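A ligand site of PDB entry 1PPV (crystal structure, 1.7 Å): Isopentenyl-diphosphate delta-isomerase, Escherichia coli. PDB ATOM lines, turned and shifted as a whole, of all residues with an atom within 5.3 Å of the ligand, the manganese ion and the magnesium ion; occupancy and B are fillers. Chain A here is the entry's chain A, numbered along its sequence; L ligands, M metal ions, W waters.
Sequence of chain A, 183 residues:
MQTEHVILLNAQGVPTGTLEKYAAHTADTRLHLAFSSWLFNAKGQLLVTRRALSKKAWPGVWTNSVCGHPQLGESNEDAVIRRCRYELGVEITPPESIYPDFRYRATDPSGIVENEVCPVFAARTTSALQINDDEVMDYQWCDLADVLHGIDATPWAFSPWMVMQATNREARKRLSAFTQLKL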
ATOM      1  N   GLU A   4     -23.825  -7.669  -0.195  1.00  0.00           N
ATOM      2  CA  GLU A   4     -23.465  -9.072  -0.035  1.00  0.00           C
ATOM      3  C   GLU A   4     -22.558  -9.514  -1.180  1.00  0.00           C
ATOM      4  O   GLU A   4     -22.624  -9.012  -2.306  1.00  0.00           O
ATOM      5  CB  GLU A   4     -24.688 -10.008   0.049  1.00  0.00           C
ATOM      6  CG  GLU A   4     -24.361 -11.385   0.613  1.00  0.00           C
ATOM      7  CD  GLU A   4     -25.545 -12.277   0.963  1.00  0.00           C
ATOM      8  OE1 GLU A   4     -26.693 -11.814   0.737  1.00  0.00           O
ATOM      9  OE2 GLU A   4     -25.350 -13.428   1.452  1.00  0.00           O
ATOM     10  N   VAL A   6     -20.140 -13.099  -2.875  1.00  0.00           N
ATOM     11  CA  VAL A   6     -19.780 -14.511  -2.839  1.00  0.00           C
ATOM     12  C   VAL A   6     -18.244 -14.580  -2.787  1.00  0.00           C
ATOM     13  O   VAL A   6     -17.561 -13.638  -3.208  1.00  0.00           O
ATOM     14  CB  VAL A   6     -20.272 -15.378  -4.000  1.00  0.00           C
ATOM     15  CG1 VAL A   6     -21.780 -15.127  -4.197  1.00  0.00           C
ATOM     16  CG2 VAL A   6     -19.494 -15.109  -5.281  1.00  0.00           C
ATOM     17  N   LYS A  21     -22.864 -10.285  -5.037  1.00  0.00           N
ATOM     18  CA  LYS A  21     -23.624 -11.528  -5.169  1.00  0.00           C
ATOM     19  C   LYS A  21     -24.456 -11.581  -6.446  1.00  0.00           C
ATOM     20  O   LYS A  21     -24.486 -12.576  -7.177  1.00  0.00           O
ATOM     21  CB  LYS A  21     -24.504 -11.743  -3.924  1.00  0.00           C
ATOM     22  CG  LYS A  21     -25.251 -13.076  -3.945  1.00  0.00           C
ATOM     23  CD  LYS A  21     -25.968 -13.340  -2.630  1.00  0.00           C
ATOM     24  CE  LYS A  21     -27.357 -12.701  -2.685  1.00  0.00           C
ATOM     25  NZ  LYS A  21     -28.092 -12.956  -1.401  1.00  0.00           N
ATOM     26  N   HIS A  25     -23.639 -14.404 -10.501  1.00  0.00           N
ATOM     27  CA  HIS A  25     -24.382 -15.545 -11.039  1.00  0.00           C
ATOM     28  C   HIS A  25     -24.831 -15.198 -12.453  1.00  0.00           C
ATOM     29  O   HIS A  25     -25.685 -14.313 -12.636  1.00  0.00           O
ATOM     30  CB  HIS A  25     -25.560 -15.831 -10.119  1.00  0.00           C
ATOM     31  CG  HIS A  25     -25.169 -16.308  -8.759  1.00  0.00           C
ATOM     32  ND1 HIS A  25     -25.088 -15.515  -7.641  1.00  0.00           N
ATOM     33  CD2 HIS A  25     -24.812 -17.538  -8.348  1.00  0.00           C
ATOM     34  CE1 HIS A  25     -24.714 -16.261  -6.620  1.00  0.00           C
ATOM     35  NE2 HIS A  25     -24.528 -17.524  -6.995  1.00  0.00           N
ATOM     36  N   HIS A  32     -17.542 -20.804  -6.365  1.00  0.00           N
ATOM     37  CA  HIS A  32     -17.596 -20.012  -5.136  1.00  0.00           C
ATOM     38  C   HIS A  32     -18.234 -20.809  -4.004  1.00  0.00           C
ATOM     39  O   HIS A  32     -18.742 -21.914  -4.176  1.00  0.00           O
ATOM     40  CB  HIS A  32     -18.323 -18.696  -5.367  1.00  0.00           C
ATOM     41  CG  HIS A  32     -19.762 -18.843  -5.738  1.00  0.00           C
ATOM     42  ND1 HIS A  32     -20.142 -19.011  -7.061  1.00  0.00           N
ATOM     43  CD2 HIS A  32     -20.899 -18.824  -5.007  1.00  0.00           C
ATOM     44  CE1 HIS A  32     -21.462 -19.110  -7.124  1.00  0.00           C
ATOM     45  NE2 HIS A  32     -21.949 -19.008  -5.897  1.00  0.00           N
ATOM     46  N   ALA A  34     -20.799 -21.809  -0.926  1.00  0.00           N
ATOM     47  CA  ALA A  34     -22.215 -21.745  -0.602  1.00  0.00           C
ATOM     48  C   ALA A  34     -22.577 -22.703   0.507  1.00  0.00           C
ATOM     49  O   ALA A  34     -21.749 -23.519   0.906  1.00  0.00           O
ATOM     50  CB  ALA A  34     -23.011 -22.112  -1.842  1.00  0.00           C
ATOM     51  N   PHE A  35     -23.827 -22.684   0.972  1.00  0.00           N
ATOM     52  CA  PHE A  35     -24.249 -23.752   1.859  1.00  0.00           C
ATOM     53  C   PHE A  35     -25.657 -24.194   1.414  1.00  0.00           C
ATOM     54  O   PHE A  35     -26.359 -23.393   0.800  1.00  0.00           O
ATOM     55  CB  PHE A  35     -24.317 -23.388   3.353  1.00  0.00           C
ATOM     56  CG  PHE A  35     -25.385 -22.342   3.676  1.00  0.00           C
ATOM     57  CD1 PHE A  35     -26.671 -22.653   4.091  1.00  0.00           C
ATOM     58  CD2 PHE A  35     -25.041 -21.006   3.521  1.00  0.00           C
ATOM     59  CE1 PHE A  35     -27.625 -21.676   4.322  1.00  0.00           C
ATOM     60  CE2 PHE A  35     -25.990 -20.024   3.792  1.00  0.00           C
ATOM     61  CZ  PHE A  35     -27.271 -20.349   4.194  1.00  0.00           C
ATOM     62  N   SER A  36     -26.029 -25.378   1.847  1.00  0.00           N
ATOM     63  CA  SER A  36     -27.441 -25.777   1.742  1.00  0.00           C
ATOM     64  C   SER A  36     -27.943 -26.302   3.066  1.00  0.00           C
ATOM     65  O   SER A  36     -27.226 -26.927   3.862  1.00  0.00           O
ATOM     66  CB  SER A  36     -27.565 -26.795   0.598  1.00  0.00           C
ATOM     67  OG  SER A  36     -28.842 -27.399   0.561  1.00  0.00           O
ATOM     68  N   ARG A  51     -38.697 -21.300  -4.449  1.00  0.00           N
ATOM     69  CA  ARG A  51     -37.970 -20.051  -4.617  1.00  0.00           C
ATOM     70  C   ARG A  51     -38.835 -18.975  -5.278  1.00  0.00           C
ATOM     71  O   ARG A  51     -39.555 -19.271  -6.236  1.00  0.00           O
ATOM     72  CB  ARG A  51     -36.719 -20.337  -5.460  1.00  0.00           C
ATOM     73  CG  ARG A  51     -35.703 -21.194  -4.695  1.00  0.00           C
ATOM     74  CD  ARG A  51     -34.601 -21.634  -5.663  1.00  0.00           C
ATOM     75  NE  ARG A  51     -33.737 -20.553  -6.108  1.00  0.00           N
ATOM     76  CZ  ARG A  51     -32.774 -20.014  -5.361  1.00  0.00           C
ATOM     77  NH1 ARG A  51     -32.567 -20.454  -4.126  1.00  0.00           N
ATOM     78  NH2 ARG A  51     -32.039 -19.040  -5.897  1.00  0.00           N
ATOM     79  N   LYS A  55     -35.862 -14.593  -7.856  1.00  0.00           N
ATOM     80  CA  LYS A  55     -34.497 -15.123  -7.684  1.00  0.00           C
ATOM     81  C   LYS A  55     -33.777 -15.191  -9.016  1.00  0.00           C
ATOM     82  O   LYS A  55     -34.338 -15.601 -10.046  1.00  0.00           O
ATOM     83  CB  LYS A  55     -34.500 -16.489  -7.010  1.00  0.00           C
ATOM     84  CG  LYS A  55     -35.017 -16.516  -5.577  1.00  0.00           C
ATOM     85  CD  LYS A  55     -34.236 -15.575  -4.673  1.00  0.00           C
ATOM     86  CE  LYS A  55     -32.799 -15.975  -4.427  1.00  0.00           C
ATOM     87  NZ  LYS A  55     -32.162 -15.064  -3.418  1.00  0.00           N
ATOM     88  N   VAL A  66     -33.317 -23.952   2.903  1.00  0.00           N
ATOM     89  CA  VAL A  66     -32.664 -22.656   2.836  1.00  0.00           C
ATOM     90  C   VAL A  66     -31.242 -22.882   2.308  1.00  0.00           C
ATOM     91  O   VAL A  66     -30.635 -23.845   2.798  1.00  0.00           O
ATOM     92  CB  VAL A  66     -32.566 -21.973   4.205  1.00  0.00           C
ATOM     93  CG1 VAL A  66     -31.919 -22.916   5.208  1.00  0.00           C
ATOM     94  CG2 VAL A  66     -31.754 -20.682   4.176  1.00  0.00           C
ATOM     95  N   CYS A  67     -30.833 -22.053   1.378  1.00  0.00           N
ATOM     96  CA  CYS A  67     -29.565 -22.070   0.697  1.00  0.00           C
ATOM     97  C   CYS A  67     -28.963 -20.671   0.757  1.00  0.00           C
ATOM     98  O   CYS A  67     -29.689 -19.686   0.817  1.00  0.00           O
ATOM     99  CB  CYS A  67     -29.647 -22.415  -0.802  1.00  0.00           C
ATOM    100  SG  CYS A  67     -29.648 -24.184  -1.151  1.00  0.00           S
ATOM    101  N   GLY A  68     -27.619 -20.576   0.715  1.00  0.00           N
ATOM    102  CA  GLY A  68     -27.064 -19.240   0.775  1.00  0.00           C
ATOM    103  C   GLY A  68     -25.538 -19.261   0.554  1.00  0.00           C
ATOM    104  O   GLY A  68     -24.964 -20.280   0.187  1.00  0.00           O
ATOM    105  N   HIS A  69     -24.967 -18.103   0.786  1.00  0.00           N
ATOM    106  CA  HIS A  69     -23.585 -17.791   0.451  1.00  0.00           C
ATOM    107  C   HIS A  69     -22.871 -17.195   1.678  1.00  0.00           C
ATOM    108  O   HIS A  69     -23.123 -16.050   2.044  1.00  0.00           O
ATOM    109  CB  HIS A  69     -23.558 -16.788  -0.687  1.00  0.00           C
ATOM    110  CG  HIS A  69     -24.067 -17.307  -1.999  1.00  0.00           C
ATOM    111  ND1 HIS A  69     -25.369 -17.079  -2.446  1.00  0.00           N
ATOM    112  CD2 HIS A  69     -23.454 -18.054  -2.951  1.00  0.00           C
ATOM    113  CE1 HIS A  69     -25.523 -17.677  -3.629  1.00  0.00           C
ATOM    114  NE2 HIS A  69     -24.367 -18.272  -3.960  1.00  0.00           N
ATOM    115  N   ARG A  83     -29.333 -16.831   7.116  1.00  0.00           N
ATOM    116  CA  ARG A  83     -30.352 -16.895   6.043  1.00  0.00           C
ATOM    117  C   ARG A  83     -31.638 -17.529   6.549  1.00  0.00           C
ATOM    118  O   ARG A  83     -32.703 -17.223   5.969  1.00  0.00           O
ATOM    119  CB  ARG A  83     -29.787 -17.666   4.845  1.00  0.00           C
ATOM    120  CG  ARG A  83     -28.694 -16.946   4.087  1.00  0.00           C
ATOM    121  CD  ARG A  83     -29.037 -15.533   3.688  1.00  0.00           C
ATOM    122  NE  ARG A  83     -29.957 -15.518   2.545  1.00  0.00           N
ATOM    123  CZ  ARG A  83     -30.180 -14.408   1.864  1.00  0.00           C
ATOM    124  NH1 ARG A  83     -29.573 -13.277   2.211  1.00  0.00           N
ATOM    125  NH2 ARG A  83     -31.007 -14.400   0.807  1.00  0.00           N
ATOM    126  N   GLU A  87     -34.601 -15.228   5.286  1.00  0.00           N
ATOM    127  CA  GLU A  87     -35.550 -15.729   4.283  1.00  0.00           C
ATOM    128  C   GLU A  87     -36.847 -16.226   4.928  1.00  0.00           C
ATOM    129  O   GLU A  87     -37.935 -16.089   4.333  1.00  0.00           O
ATOM    130  CB  GLU A  87     -34.916 -16.900   3.489  1.00  0.00           C
ATOM    131  CG  GLU A  87     -33.603 -16.521   2.794  1.00  0.00           C
ATOM    132  CD  GLU A  87     -33.045 -17.647   1.953  1.00  0.00           C
ATOM    133  OE1 GLU A  87     -33.708 -18.692   1.792  1.00  0.00           O
ATOM    134  OE2 GLU A  87     -31.904 -17.504   1.430  1.00  0.00           O
ATOM    135  N   TYR A 104     -21.102 -28.870  -6.739  1.00  0.00           N
ATOM    136  CA  TYR A 104     -21.813 -29.197  -7.971  1.00  0.00           C
ATOM    137  C   TYR A 104     -21.813 -28.016  -8.930  1.00  0.00           C
ATOM    138  O   TYR A 104     -21.578 -26.892  -8.530  1.00  0.00           O
ATOM    139  CB  TYR A 104     -23.264 -29.598  -7.661  1.00  0.00           C
ATOM    140  CG  TYR A 104     -24.106 -28.355  -7.435  1.00  0.00           C
ATOM    141  CD1 TYR A 104     -25.052 -27.918  -8.352  1.00  0.00           C
ATOM    142  CD2 TYR A 104     -23.904 -27.616  -6.273  1.00  0.00           C
ATOM    143  CE1 TYR A 104     -25.813 -26.782  -8.148  1.00  0.00           C
ATOM    144  CE2 TYR A 104     -24.668 -26.473  -6.062  1.00  0.00           C
ATOM    145  CZ  TYR A 104     -25.599 -26.064  -6.989  1.00  0.00           C
ATOM    146  OH  TYR A 104     -26.347 -24.929  -6.764  1.00  0.00           O
ATOM    147  N   GLU A 114     -25.125 -22.221 -11.449  1.00  0.00           N
ATOM    148  CA  GLU A 114     -24.563 -22.214 -10.084  1.00  0.00           C
ATOM    149  C   GLU A 114     -23.381 -23.198 -10.114  1.00  0.00           C
ATOM    150  O   GLU A 114     -23.478 -24.253 -10.722  1.00  0.00           O
ATOM    151  CB  GLU A 114     -25.524 -22.605  -8.972  1.00  0.00           C
ATOM    152  CG  GLU A 114     -26.330 -21.464  -8.362  1.00  0.00           C
ATOM    153  CD  GLU A 114     -25.501 -20.611  -7.425  1.00  0.00           C
ATOM    154  OE1 GLU A 114     -26.078 -19.911  -6.559  1.00  0.00           O
ATOM    155  OE2 GLU A 114     -24.245 -20.629  -7.578  1.00  0.00           O
ATOM    156  N   GLU A 116     -20.627 -24.343  -7.254  1.00  0.00           N
ATOM    157  CA  GLU A 116     -20.415 -24.139  -5.842  1.00  0.00           C
ATOM    158  C   GLU A 116     -19.796 -25.337  -5.153  1.00  0.00           C
ATOM    159  O   GLU A 116     -20.062 -26.496  -5.383  1.00  0.00           O
ATOM    160  CB  GLU A 116     -21.744 -23.825  -5.117  1.00  0.00           C
ATOM    161  CG  GLU A 116     -22.331 -22.483  -5.540  1.00  0.00           C
ATOM    162  CD  GLU A 116     -23.728 -22.193  -5.038  1.00  0.00           C
ATOM    163  OE1 GLU A 116     -24.370 -23.185  -4.640  1.00  0.00           O
ATOM    164  OE2 GLU A 116     -24.118 -20.987  -5.025  1.00  0.00           O
ATOM    165  N   CYS A 118     -20.415 -26.617  -1.634  1.00  0.00           N
ATOM    166  CA  CYS A 118     -21.664 -26.361  -0.922  1.00  0.00           C
ATOM    167  C   CYS A 118     -21.949 -27.376   0.157  1.00  0.00           C
ATOM    168  O   CYS A 118     -22.772 -28.284   0.000  1.00  0.00           O
ATOM    169  CB  CYS A 118     -22.799 -26.359  -1.974  1.00  0.00           C
ATOM    170  SG  CYS A 118     -24.422 -25.960  -1.243  1.00  0.00           S
ATOM    171  N   GLU A 135     -37.822 -13.820  -1.184  1.00  0.00           N
ATOM    172  CA  GLU A 135     -37.004 -15.035  -1.227  1.00  0.00           C
ATOM    173  C   GLU A 135     -37.829 -16.292  -1.488  1.00  0.00           C
ATOM    174  O   GLU A 135     -37.407 -17.155  -2.265  1.00  0.00           O
ATOM    175  CB  GLU A 135     -36.249 -15.224   0.102  1.00  0.00           C
ATOM    176  CG  GLU A 135     -35.266 -14.100   0.413  1.00  0.00           C
ATOM    177  CD  GLU A 135     -34.137 -13.993  -0.611  1.00  0.00           C
ATOM    178  OE1 GLU A 135     -33.710 -15.036  -1.144  1.00  0.00           O
ATOM    179  OE2 GLU A 135     -33.666 -12.867  -0.903  1.00  0.00           O
ATOM    180  N   TRP A 161     -29.774 -29.379  -7.159  1.00  0.00           N
ATOM    181  CA  TRP A 161     -28.955 -29.634  -5.959  1.00  0.00           C
ATOM    182  C   TRP A 161     -29.730 -30.347  -4.877  1.00  0.00           C
ATOM    183  O   TRP A 161     -29.192 -31.123  -4.087  1.00  0.00           O
ATOM    184  CB  TRP A 161     -28.351 -28.340  -5.438  1.00  0.00           C
ATOM    185  CG  TRP A 161     -29.331 -27.362  -4.895  1.00  0.00           C
ATOM    186  CD1 TRP A 161     -29.863 -27.274  -3.642  1.00  0.00           C
ATOM    187  CD2 TRP A 161     -29.901 -26.275  -5.659  1.00  0.00           C
ATOM    188  NE1 TRP A 161     -30.738 -26.200  -3.582  1.00  0.00           N
ATOM    189  CE2 TRP A 161     -30.771 -25.582  -4.797  1.00  0.00           C
ATOM    190  CE3 TRP A 161     -29.728 -25.855  -6.990  1.00  0.00           C
ATOM    191  CZ2 TRP A 161     -31.502 -24.463  -5.214  1.00  0.00           C
ATOM    192  CZ3 TRP A 161     -30.453 -24.744  -7.396  1.00  0.00           C
ATOM    193  CH2 TRP A 161     -31.307 -24.073  -6.522  1.00  0.00           C
HETATM  194  O1  LIG L   1     -28.322 -22.191  -4.894  1.00  0.00           O
HETATM  195  O2  LIG L   1     -29.535 -15.613  -2.687  1.00  0.00           O
HETATM  196  O3  LIG L   1     -27.804 -15.949  -1.106  1.00  0.00           O
HETATM  197  O4  LIG L   1     -30.054 -16.782  -0.688  1.00  0.00           O
HETATM  198  P1  LIG L   1     -29.067 -16.485  -1.768  1.00  0.00           P
HETATM  199  O5  LIG L   1     -28.611 -17.798  -2.443  1.00  0.00           O
HETATM  200  O6  LIG L   1     -29.443 -18.902  -4.324  1.00  0.00           O
HETATM  201  O7  LIG L   1     -30.612 -19.209  -2.228  1.00  0.00           O
HETATM  202  P2  LIG L   1     -29.332 -19.039  -2.991  1.00  0.00           P
HETATM  203  C1  LIG L   1     -25.776 -22.837  -5.012  1.00  0.00           C
HETATM  204  C2  LIG L   1     -27.238 -24.146  -3.492  1.00  0.00           C
HETATM  205  C3  LIG L   1     -27.282 -20.424  -3.249  1.00  0.00           C
HETATM  206  C4  LIG L   1     -26.626 -21.778  -2.934  1.00  0.00           C
HETATM  207  C5  LIG L   1     -27.035 -22.731  -4.093  1.00  0.00           C
HETATM  208  O8  LIG L   1     -28.515 -20.254  -2.532  1.00  0.00           O
HETATM  209 MN    MN M   1     -24.094 -19.197  -5.854  1.00  0.00          MN
HETATM  210 MG    MG M   2     -31.239 -18.473  -0.340  1.00  0.00          MG
HETATM  211  O   HOH W   1     -26.764 -15.959   1.364  1.00  0.00           O
HETATM  212  O   HOH W   2     -27.767 -15.246  -5.052  1.00  0.00           O
HETATM  213  O   HOH W   3     -28.034 -17.949  -6.435  1.00  0.00           O
HETATM  214  O   HOH W   4     -33.101 -17.572  -1.289  1.00  0.00           O
HETATM  215  O   HOH W   5     -32.430 -20.067   0.054  1.00  0.00           O
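The manganese ion is bound by the side-chain carboxylate (OE2) of Glu 116 (2.0 Å), a ring nitrogen (NE2) of His 25 (2.1 Å), a ring nitrogen (NE2) of His 69 (2.1 Å), a ring nitrogen (NE2) of His 32 (2.2 Å), the side-chain carboxylate (OE1) of Glu 114 (2.2 Å) and the side-chain carboxylate (OE2) of Glu 114 (2.2 Å).
Water W5 lies within hydrogen-bond range of OE1 of Glu 87 (2.6 Å) and N of Cys 67 (2.9 Å). Water W4 lies within hydrogen-bond range of OE1 of Glu 135 (2.6 Å), OE1 of Glu 87 (3.3 Å) and NZ of Lys 55 (3.4 Å). Water W1 lies within hydrogen-bond range of O3 of the ligand (2.7 Å), N of His 69 (2.9 Å), OE2 of Glu 4 (2.9 Å) and NE of Arg 83 (3.4 Å).
Water W5 is bound to the magnesium ion (2.0 Å). O4 of the ligand is bound to the magnesium ion, 2.1 Å away. O7 of the ligand is bound to the magnesium ion. The magnesium ion is bound by OE2 of Glu 87, 2.1 Å away. The magnesium ion is bound by water W4 (2.3 Å). The magnesium ion is bound by the backbone carbonyl oxygen (O) of Cys 67 (2.3 Å). The magnesium ion has six donor atoms within binding distance.
CB of Ala 34 touches C4 of the ligand, at 3.8 Å. OH of Tyr 104 touches C1 of the ligand, 2.8 Å away. CH2 of Trp 161 touches O1 of the ligand, 3.9 Å away. Hydrophobic or aromatic side chains that line the ligand: Ala 34, His 69, Tyr 104 and Trp 161. Of the 22 residues printed, 13 come within 4 Å of the ligand.
Five residues have an atom within 4 Å of the manganese ion: His 25, His 32, His 69, Glu 114 and Glu 116.
NZ of Lys 21 lies within salt-bridge range of OE1 of Glu 4 (2.8 Å). O of Gly 68 sits at hydrogen-bond distance from N of Phe 35. The side-chain sulfur (SG) of Cys 67 is in hydrogen-bond range of the indole nitrogen (NE1) of Trp 161 (3.3 Å). The side-chain carboxylate (OE1) of Glu 135 lies within salt-bridge range of the guanidinium group (NH2) of Arg 83 (3.4 Å). OE2 of Glu 87 sits close to NE of Arg 83 (3.0 Å). A ring nitrogen (ND1) of His 25 lies within hydrogen-bond range of the backbone carbonyl oxygen (O) of Lys 21, at 3.0 Å. SG of Cys 67 lies within hydrogen-bond range of OG of Ser 36 (3.7 Å). The guanidinium group (NH1) of Arg 83 lies within salt-bridge range of the side-chain carboxylate (OE1) of Glu 4 (3.6 Å).
Within 4 Å of the magnesium ion: Cys 67 and Glu 87. The nearest printed residue that does not touch the magnesium ion is Arg 83 (4.2 Å).
A carbon (C1) of the ligand is covalently linked to the side-chain carboxylate (OE1) of Glu 116, at 1.5 Å. An oxygen (O3) of the ligand lies within salt-bridge range of the side-chain amino group (NZ) of Lys 21. NH2 of Arg 83 lies within salt-bridge range of O2 of the ligand, at 3.98 Å. A ring nitrogen (ND1) of His 69 lies within hydrogen-bond range of an oxygen (O3) of the ligand, at 3.0 Å. The guanidinium group (NH2) of Arg 51 is in salt-bridge range of an oxygen (O6) of the ligand, 3.0 Å away. The backbone NH of Gly 68 is in hydrogen-bond range of an oxygen (O8) of the ligand (3.4 Å). An oxygen (O2) of the ligand is in salt-bridge range of the side-chain amino group of Lys 55, 2.8 Å away.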
